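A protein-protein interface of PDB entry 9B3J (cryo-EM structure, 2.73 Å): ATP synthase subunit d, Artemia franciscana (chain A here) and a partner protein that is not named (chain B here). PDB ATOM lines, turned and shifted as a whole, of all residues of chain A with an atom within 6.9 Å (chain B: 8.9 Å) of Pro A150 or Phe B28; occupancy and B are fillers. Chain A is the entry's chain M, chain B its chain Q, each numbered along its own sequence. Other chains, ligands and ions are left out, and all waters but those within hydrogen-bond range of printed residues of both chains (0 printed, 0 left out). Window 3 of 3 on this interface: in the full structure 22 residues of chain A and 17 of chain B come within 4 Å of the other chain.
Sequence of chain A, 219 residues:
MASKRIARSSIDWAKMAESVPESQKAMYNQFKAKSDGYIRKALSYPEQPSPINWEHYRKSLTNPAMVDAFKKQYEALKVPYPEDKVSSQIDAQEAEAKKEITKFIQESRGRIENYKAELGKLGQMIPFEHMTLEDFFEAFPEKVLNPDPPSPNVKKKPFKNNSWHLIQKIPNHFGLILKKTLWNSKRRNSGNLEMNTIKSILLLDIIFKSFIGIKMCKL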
ATOM      1  N   VAL A 144     -13.956 -15.765  22.225  1.00  0.00           N
ATOM      2  CA  VAL A 144     -14.783 -14.669  21.737  1.00  0.00           C
ATOM      3  C   VAL A 144     -15.750 -14.317  22.862  1.00  0.00           C
ATOM      4  O   VAL A 144     -16.502 -15.172  23.340  1.00  0.00           O
ATOM      5  CB  VAL A 144     -15.505 -15.032  20.424  1.00  0.00           C
ATOM      6  CG1 VAL A 144     -16.000 -16.475  20.440  1.00  0.00           C
ATOM      7  CG2 VAL A 144     -16.645 -14.065  20.156  1.00  0.00           C
ATOM      8  N   LEU A 145     -15.715 -13.070  23.317  1.00  0.00           N
ATOM      9  CA  LEU A 145     -16.398 -12.676  24.540  1.00  0.00           C
ATOM     10  C   LEU A 145     -17.456 -11.626  24.239  1.00  0.00           C
ATOM     11  O   LEU A 145     -17.523 -11.071  23.141  1.00  0.00           O
ATOM     12  CB  LEU A 145     -15.399 -12.146  25.576  1.00  0.00           C
ATOM     13  CG  LEU A 145     -15.715 -12.429  27.045  1.00  0.00           C
ATOM     14  CD1 LEU A 145     -15.989 -13.908  27.249  1.00  0.00           C
ATOM     15  CD2 LEU A 145     -14.571 -11.965  27.931  1.00  0.00           C
ATOM     16  N   ASN A 146     -18.309 -11.379  25.235  1.00  0.00           N
ATOM     17  CA  ASN A 146     -19.333 -10.344  25.102  1.00  0.00           C
ATOM     18  C   ASN A 146     -18.756  -8.934  24.970  1.00  0.00           C
ATOM     19  O   ASN A 146     -19.215  -8.195  24.082  1.00  0.00           O
ATOM     20  CB  ASN A 146     -20.332 -10.472  26.258  1.00  0.00           C
ATOM     21  CG  ASN A 146     -20.657 -11.913  26.577  1.00  0.00           C
ATOM     22  OD1 ASN A 146     -20.413 -12.803  25.768  1.00  0.00           O
ATOM     23  ND2 ASN A 146     -21.203 -12.151  27.762  1.00  0.00           N
ATOM     24  N   ASP A 148     -16.222  -7.869  23.342  1.00  0.00           N
ATOM     25  CA  ASP A 148     -15.197  -8.101  22.337  1.00  0.00           C
ATOM     26  C   ASP A 148     -15.751  -7.698  20.980  1.00  0.00           C
ATOM     27  O   ASP A 148     -16.973  -7.712  20.783  1.00  0.00           O
ATOM     28  CB  ASP A 148     -14.759  -9.578  22.329  1.00  0.00           C
ATOM     29  CG  ASP A 148     -13.450  -9.811  21.590  1.00  0.00           C
ATOM     30  OD1 ASP A 148     -13.465  -9.864  20.342  1.00  0.00           O
ATOM     31  OD2 ASP A 148     -12.403  -9.939  22.257  1.00  0.00           O
ATOM     32  N   PRO A 149     -14.891  -7.277  20.053  1.00  0.00           N
ATOM     33  CA  PRO A 149     -15.333  -7.022  18.677  1.00  0.00           C
ATOM     34  C   PRO A 149     -15.929  -8.264  18.040  1.00  0.00           C
ATOM     35  O   PRO A 149     -15.244  -9.282  17.859  1.00  0.00           O
ATOM     36  CB  PRO A 149     -14.039  -6.599  17.972  1.00  0.00           C
ATOM     37  CG  PRO A 149     -13.280  -5.911  19.031  1.00  0.00           C
ATOM     38  CD  PRO A 149     -13.586  -6.644  20.317  1.00  0.00           C
ATOM     39  N   PRO A 150     -17.204  -8.210  17.682  1.00  0.00           N
ATOM     40  CA  PRO A 150     -17.896  -9.409  17.207  1.00  0.00           C
ATOM     41  C   PRO A 150     -17.918  -9.548  15.695  1.00  0.00           C
ATOM     42  O   PRO A 150     -17.480  -8.649  14.972  1.00  0.00           O
ATOM     43  CB  PRO A 150     -19.311  -9.212  17.760  1.00  0.00           C
ATOM     44  CG  PRO A 150     -19.455  -7.684  17.939  1.00  0.00           C
ATOM     45  CD  PRO A 150     -18.108  -7.050  17.738  1.00  0.00           C
ATOM     46  N   SER A 151     -18.428 -10.694  15.223  1.00  0.00           N
ATOM     47  CA  SER A 151     -18.752 -11.006  13.833  1.00  0.00           C
ATOM     48  C   SER A 151     -19.475 -12.348  13.770  1.00  0.00           C
ATOM     49  O   SER A 151     -19.269 -13.196  14.646  1.00  0.00           O
ATOM     50  CB  SER A 151     -17.497 -11.046  12.964  1.00  0.00           C
ATOM     51  OG  SER A 151     -16.942  -9.748  12.854  1.00  0.00           O
ATOM     52  N   PRO A 152     -20.349 -12.572  12.782  1.00  0.00           N
ATOM     53  CA  PRO A 152     -20.905 -13.922  12.596  1.00  0.00           C
ATOM     54  C   PRO A 152     -19.860 -14.933  12.189  1.00  0.00           C
ATOM     55  O   PRO A 152     -20.007 -16.124  12.488  1.00  0.00           O
ATOM     56  CB  PRO A 152     -21.943 -13.725  11.489  1.00  0.00           C
ATOM     57  CG  PRO A 152     -21.443 -12.557  10.736  1.00  0.00           C
ATOM     58  CD  PRO A 152     -20.839 -11.638  11.757  1.00  0.00           C
ATOM     59  N   ASN A 153     -18.834 -14.486  11.474  1.00  0.00           N
ATOM     60  CA  ASN A 153     -17.626 -15.248  11.194  1.00  0.00           C
ATOM     61  C   ASN A 153     -16.543 -14.600  12.038  1.00  0.00           C
ATOM     62  O   ASN A 153     -15.893 -13.649  11.606  1.00  0.00           O
ATOM     63  CB  ASN A 153     -17.277 -15.214   9.724  1.00  0.00           C
ATOM     64  CG  ASN A 153     -17.675 -13.914   9.063  1.00  0.00           C
ATOM     65  OD1 ASN A 153     -18.461 -13.903   8.117  1.00  0.00           O
ATOM     66  ND2 ASN A 153     -17.142 -12.807   9.560  1.00  0.00           N
ATOM     67  N   VAL A 154     -16.357 -15.113  13.248  1.00  0.00           N
ATOM     68  CA  VAL A 154     -15.438 -14.474  14.175  1.00  0.00           C
ATOM     69  C   VAL A 154     -14.035 -14.798  13.691  1.00  0.00           C
ATOM     70  O   VAL A 154     -13.458 -15.828  14.051  1.00  0.00           O
ATOM     71  CB  VAL A 154     -15.671 -14.951  15.618  1.00  0.00           C
ATOM     72  CG1 VAL A 154     -15.193 -13.905  16.595  1.00  0.00           C
ATOM     73  CG2 VAL A 154     -17.131 -15.257  15.850  1.00  0.00           C
ATOM     74  N   LYS A 155     -13.481 -13.908  12.882  1.00  0.00           N
ATOM     75  CA  LYS A 155     -12.268 -14.155  12.128  1.00  0.00           C
ATOM     76  C   LYS A 155     -11.154 -13.253  12.645  1.00  0.00           C
ATOM     77  O   LYS A 155     -11.312 -12.542  13.644  1.00  0.00           O
ATOM     78  CB  LYS A 155     -12.536 -13.934  10.639  1.00  0.00           C
ATOM     79  CG  LYS A 155     -11.865 -14.928   9.721  1.00  0.00           C
ATOM     80  CD  LYS A 155     -11.651 -14.326   8.345  1.00  0.00           C
ATOM     81  CE  LYS A 155     -12.950 -13.829   7.750  1.00  0.00           C
ATOM     82  NZ  LYS A 155     -13.909 -14.943   7.545  1.00  0.00           N
ATOM     83  N   PRO A 158     -12.545  -9.433  10.489  1.00  0.00           N
ATOM     84  CA  PRO A 158     -13.865  -8.949  10.068  1.00  0.00           C
ATOM     85  C   PRO A 158     -14.286  -7.633  10.711  1.00  0.00           C
ATOM     86  O   PRO A 158     -15.305  -7.056  10.319  1.00  0.00           O
ATOM     87  CB  PRO A 158     -14.794 -10.094  10.484  1.00  0.00           C
ATOM     88  CG  PRO A 158     -14.098 -10.745  11.643  1.00  0.00           C
ATOM     89  CD  PRO A 158     -12.682 -10.240  11.717  1.00  0.00           C
ATOM     90  N   PHE A 159     -13.526  -7.141  11.687  1.00  0.00           N
ATOM     91  CA  PHE A 159     -13.879  -5.939  12.423  1.00  0.00           C
ATOM     92  C   PHE A 159     -12.772  -4.904  12.304  1.00  0.00           C
ATOM     93  O   PHE A 159     -11.603  -5.239  12.086  1.00  0.00           O
ATOM     94  CB  PHE A 159     -14.151  -6.240  13.906  1.00  0.00           C
ATOM     95  CG  PHE A 159     -13.113  -7.106  14.556  1.00  0.00           C
ATOM     96  CD1 PHE A 159     -11.938  -6.563  15.049  1.00  0.00           C
ATOM     97  CD2 PHE A 159     -13.327  -8.463  14.700  1.00  0.00           C
ATOM     98  CE1 PHE A 159     -10.991  -7.359  15.650  1.00  0.00           C
ATOM     99  CE2 PHE A 159     -12.382  -9.264  15.301  1.00  0.00           C
ATOM    100  CZ  PHE A 159     -11.213  -8.712  15.778  1.00  0.00           C
ATOM    101  N   LYS A 160     -13.170  -3.644  12.473  1.00  0.00           N
ATOM    102  CA  LYS A 160     -12.302  -2.458  12.398  1.00  0.00           C
ATOM    103  C   LYS A 160     -11.678  -2.452  11.005  1.00  0.00           C
ATOM    104  O   LYS A 160     -12.428  -2.636  10.032  1.00  0.00           O
ATOM    105  CB  LYS A 160     -11.324  -2.452  13.571  1.00  0.00           C
ATOM    106  CG  LYS A 160     -11.977  -2.723  14.923  1.00  0.00           C
ATOM    107  CD  LYS A 160     -13.100  -1.736  15.218  1.00  0.00           C
ATOM    108  CE  LYS A 160     -14.447  -2.439  15.378  1.00  0.00           C
ATOM    109  NZ  LYS A 160     -14.432  -3.446  16.472  1.00  0.00           N
ATOM    110  N   TRP B  21     -34.293 -13.838  16.045  1.00  0.00           N
ATOM    111  CA  TRP B  21     -33.168 -13.541  16.923  1.00  0.00           C
ATOM    112  C   TRP B  21     -32.489 -14.810  17.421  1.00  0.00           C
ATOM    113  O   TRP B  21     -31.272 -14.821  17.629  1.00  0.00           O
ATOM    114  CB  TRP B  21     -33.622 -12.700  18.107  1.00  0.00           C
ATOM    115  CG  TRP B  21     -32.500 -12.013  18.771  1.00  0.00           C
ATOM    116  CD1 TRP B  21     -31.886 -10.880  18.354  1.00  0.00           C
ATOM    117  CD2 TRP B  21     -31.843 -12.410  19.975  1.00  0.00           C
ATOM    118  NE1 TRP B  21     -30.885 -10.540  19.223  1.00  0.00           N
ATOM    119  CE2 TRP B  21     -30.839 -11.465  20.229  1.00  0.00           C
ATOM    120  CE3 TRP B  21     -32.009 -13.467  20.866  1.00  0.00           C
ATOM    121  CZ2 TRP B  21     -30.002 -11.547  21.331  1.00  0.00           C
ATOM    122  CZ3 TRP B  21     -31.177 -13.546  21.959  1.00  0.00           C
ATOM    123  CH2 TRP B  21     -30.187 -12.593  22.183  1.00  0.00           C
ATOM    124  N   ALA B  22     -33.250 -15.885  17.621  1.00  0.00           N
ATOM    125  CA  ALA B  22     -32.629 -17.139  18.021  1.00  0.00           C
ATOM    126  C   ALA B  22     -31.783 -17.721  16.897  1.00  0.00           C
ATOM    127  O   ALA B  22     -30.723 -18.297  17.147  1.00  0.00           O
ATOM    128  CB  ALA B  22     -33.690 -18.133  18.470  1.00  0.00           C
ATOM    129  N   ILE B  23     -32.221 -17.570  15.649  1.00  0.00           N
ATOM    130  CA  ILE B  23     -31.408 -18.019  14.523  1.00  0.00           C
ATOM    131  C   ILE B  23     -30.166 -17.150  14.390  1.00  0.00           C
ATOM    132  O   ILE B  23     -29.074 -17.639  14.064  1.00  0.00           O
ATOM    133  CB  ILE B  23     -32.251 -18.035  13.236  1.00  0.00           C
ATOM    134  CG1 ILE B  23     -33.238 -19.192  13.298  1.00  0.00           C
ATOM    135  CG2 ILE B  23     -31.387 -18.157  12.002  1.00  0.00           C
ATOM    136  CD1 ILE B  23     -33.993 -19.415  12.032  1.00  0.00           C
ATOM    137  N   MET B  24     -30.305 -15.855  14.680  1.00  0.00           N
ATOM    138  CA  MET B  24     -29.161 -14.951  14.664  1.00  0.00           C
ATOM    139  C   MET B  24     -28.108 -15.367  15.680  1.00  0.00           C
ATOM    140  O   MET B  24     -26.918 -15.435  15.362  1.00  0.00           O
ATOM    141  CB  MET B  24     -29.639 -13.530  14.938  1.00  0.00           C
ATOM    142  CG  MET B  24     -28.639 -12.458  14.609  1.00  0.00           C
ATOM    143  SD  MET B  24     -29.304 -10.839  14.997  1.00  0.00           S
ATOM    144  CE  MET B  24     -30.911 -10.983  14.239  1.00  0.00           C
ATOM    145  N   THR B  25     -28.524 -15.684  16.898  1.00  0.00           N
ATOM    146  CA  THR B  25     -27.533 -16.117  17.869  1.00  0.00           C
ATOM    147  C   THR B  25     -27.100 -17.564  17.691  1.00  0.00           C
ATOM    148  O   THR B  25     -26.187 -18.000  18.394  1.00  0.00           O
ATOM    149  CB  THR B  25     -28.033 -15.939  19.291  1.00  0.00           C
ATOM    150  OG1 THR B  25     -27.071 -16.505  20.176  1.00  0.00           O
ATOM    151  CG2 THR B  25     -29.299 -16.667  19.495  1.00  0.00           C
ATOM    152  N   MET B  26     -27.753 -18.335  16.822  1.00  0.00           N
ATOM    153  CA  MET B  26     -27.197 -19.639  16.471  1.00  0.00           C
ATOM    154  C   MET B  26     -26.104 -19.510  15.419  1.00  0.00           C
ATOM    155  O   MET B  26     -25.097 -20.221  15.476  1.00  0.00           O
ATOM    156  CB  MET B  26     -28.294 -20.580  15.969  1.00  0.00           C
ATOM    157  CG  MET B  26     -29.262 -21.093  17.030  1.00  0.00           C
ATOM    158  SD  MET B  26     -28.521 -22.106  18.318  1.00  0.00           S
ATOM    159  CE  MET B  26     -28.599 -23.729  17.570  1.00  0.00           C
ATOM    160  N   VAL B  27     -26.296 -18.616  14.445  1.00  0.00           N
ATOM    161  CA  VAL B  27     -25.279 -18.378  13.423  1.00  0.00           C
ATOM    162  C   VAL B  27     -24.064 -17.681  14.015  1.00  0.00           C
ATOM    163  O   VAL B  27     -22.930 -17.924  13.584  1.00  0.00           O
ATOM    164  CB  VAL B  27     -25.894 -17.580  12.259  1.00  0.00           C
ATOM    165  CG1 VAL B  27     -24.875 -17.267  11.202  1.00  0.00           C
ATOM    166  CG2 VAL B  27     -26.997 -18.370  11.635  1.00  0.00           C
ATOM    167  N   PHE B  28     -24.268 -16.829  15.026  1.00  0.00           N
ATOM    168  CA  PHE B  28     -23.170 -16.063  15.613  1.00  0.00           C
ATOM    169  C   PHE B  28     -22.108 -16.962  16.225  1.00  0.00           C
ATOM    170  O   PHE B  28     -20.931 -16.598  16.251  1.00  0.00           O
ATOM    171  CB  PHE B  28     -23.703 -15.099  16.672  1.00  0.00           C
ATOM    172  CG  PHE B  28     -22.661 -14.177  17.234  1.00  0.00           C
ATOM    173  CD1 PHE B  28     -22.294 -13.034  16.558  1.00  0.00           C
ATOM    174  CD2 PHE B  28     -22.056 -14.447  18.447  1.00  0.00           C
ATOM    175  CE1 PHE B  28     -21.340 -12.184  17.077  1.00  0.00           C
ATOM    176  CE2 PHE B  28     -21.101 -13.602  18.966  1.00  0.00           C
ATOM    177  CZ  PHE B  28     -20.747 -12.472  18.282  1.00  0.00           C
ATOM    178  N   PHE B  29     -22.485 -18.137  16.702  1.00  0.00           N
ATOM    179  CA  PHE B  29     -21.515 -19.064  17.248  1.00  0.00           C
ATOM    180  C   PHE B  29     -21.152 -20.167  16.276  1.00  0.00           C
ATOM    181  O   PHE B  29     -20.535 -21.155  16.681  1.00  0.00           O
ATOM    182  CB  PHE B  29     -22.035 -19.661  18.545  1.00  0.00           C
ATOM    183  CG  PHE B  29     -21.787 -18.800  19.734  1.00  0.00           C
ATOM    184  CD1 PHE B  29     -22.429 -17.591  19.869  1.00  0.00           C
ATOM    185  CD2 PHE B  29     -20.903 -19.199  20.712  1.00  0.00           C
ATOM    186  CE1 PHE B  29     -22.194 -16.804  20.950  1.00  0.00           C
ATOM    187  CE2 PHE B  29     -20.666 -18.410  21.796  1.00  0.00           C
ATOM    188  CZ  PHE B  29     -21.312 -17.214  21.915  1.00  0.00           C
ATOM    189  N   LEU B  30     -21.523 -20.027  15.008  1.00  0.00           N
ATOM    190  CA  LEU B  30     -21.199 -21.017  13.983  1.00  0.00           C
ATOM    191  C   LEU B  30     -19.984 -20.510  13.219  1.00  0.00           C
ATOM    192  O   LEU B  30     -20.106 -19.866  12.179  1.00  0.00           O
ATOM    193  CB  LEU B  30     -22.378 -21.258  13.054  1.00  0.00           C
ATOM    194  CG  LEU B  30     -22.231 -22.462  12.134  1.00  0.00           C
ATOM    195  CD1 LEU B  30     -22.284 -23.720  12.962  1.00  0.00           C
ATOM    196  CD2 LEU B  30     -23.304 -22.471  11.080  1.00  0.00           C
ATOM    197  N   TYR B  31     -18.802 -20.800  13.749  1.00  0.00           N
ATOM    198  CA  TYR B  31     -17.564 -20.472  13.063  1.00  0.00           C
ATOM    199  C   TYR B  31     -16.498 -21.461  13.499  1.00  0.00           C
ATOM    200  O   TYR B  31     -16.584 -22.060  14.573  1.00  0.00           O
ATOM    201  CB  TYR B  31     -17.123 -19.038  13.354  1.00  0.00           C
ATOM    202  CG  TYR B  31     -16.373 -18.885  14.650  1.00  0.00           C
ATOM    203  CD1 TYR B  31     -17.010 -19.048  15.870  1.00  0.00           C
ATOM    204  CD2 TYR B  31     -15.025 -18.569  14.652  1.00  0.00           C
ATOM    205  CE1 TYR B  31     -16.325 -18.908  17.052  1.00  0.00           C
ATOM    206  CE2 TYR B  31     -14.333 -18.425  15.826  1.00  0.00           C
ATOM    207  CZ  TYR B  31     -14.987 -18.596  17.022  1.00  0.00           C
ATOM    208  OH  TYR B  31     -14.294 -18.451  18.196  1.00  0.00           O
ATOM    209  N   GLN B  32     -15.483 -21.630  12.651  1.00  0.00           N
ATOM    210  CA  GLN B  32     -14.406 -22.556  12.957  1.00  0.00           C
ATOM    211  C   GLN B  32     -13.174 -21.777  13.372  1.00  0.00           C
ATOM    212  O   GLN B  32     -12.572 -21.096  12.530  1.00  0.00           O
ATOM    213  CB  GLN B  32     -14.088 -23.444  11.760  1.00  0.00           C
ATOM    214  CG  GLN B  32     -12.943 -24.406  12.021  1.00  0.00           C
ATOM    215  CD  GLN B  32     -13.239 -25.394  13.135  1.00  0.00           C
ATOM    216  OE1 GLN B  32     -14.382 -25.799  13.334  1.00  0.00           O
ATOM    217  NE2 GLN B  32     -12.206 -25.791  13.864  1.00  0.00           N
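Among the printed residues, pairs that only touch across the chains: Val A154 with Tyr B31 (3.2 Å), Ser A151 with Phe B28 (3.4 Å), Val A144 with Tyr B31 (3.4 Å), Pro A150 with Phe B28 (3.6 Å), Pro A152 with Val B27 (3.6 Å), Pro A152 with Leu B30 (3.8 Å) and Pro A152 with Phe B28 (3.9 Å).
Of the 12 printed residues of chain B, 4 touch a printed residue of chain A. Printed residues of chain B that touch a printed residue of chain A: Val B27, Phe B28, Leu B30 and Tyr B31. Hydrophobic or aromatic side chains of chain B that line the printed part of chain A: Phe B28 and Tyr B31. Of the 14 printed residues of chain A, 5 touch a printed residue of chain B. Hydrophobic or aromatic side chains of chain A that line the printed part of chain B: Val A144, Pro A150 and Val A154. Along chain A the printed residues that touch a printed residue of chain B span positions 144 to 154. Among the printed residues, 7 pairs touch across the chains.
Pro A150 touches one residue of chain B. Ser A151 touches just one residue of chain B: Phe B28 (3.4 Å). Of the printed residues of chain B, Pro A152 touches Val B27 (3.6 Å), Phe B28 (3.9 Å) and Leu B30 (3.8 Å). Asn A153 touches none of the printed residues of chain B. Printed residues of chain B within 4 Å of Val A154: Tyr B31 (3.2 Å). Of the printed residues of chain A, Val B27 touches Pro A152 (3.6 Å). Phe B28 touches three residues of chain A. Of the printed residues of chain A, Leu B30 touches Pro A152 (3.8 Å). Gln B32 touches none of the printed residues of chain A. The nearest printed residue of chain B that does not touch Val A144 is Phe B28 (4.6 Å).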
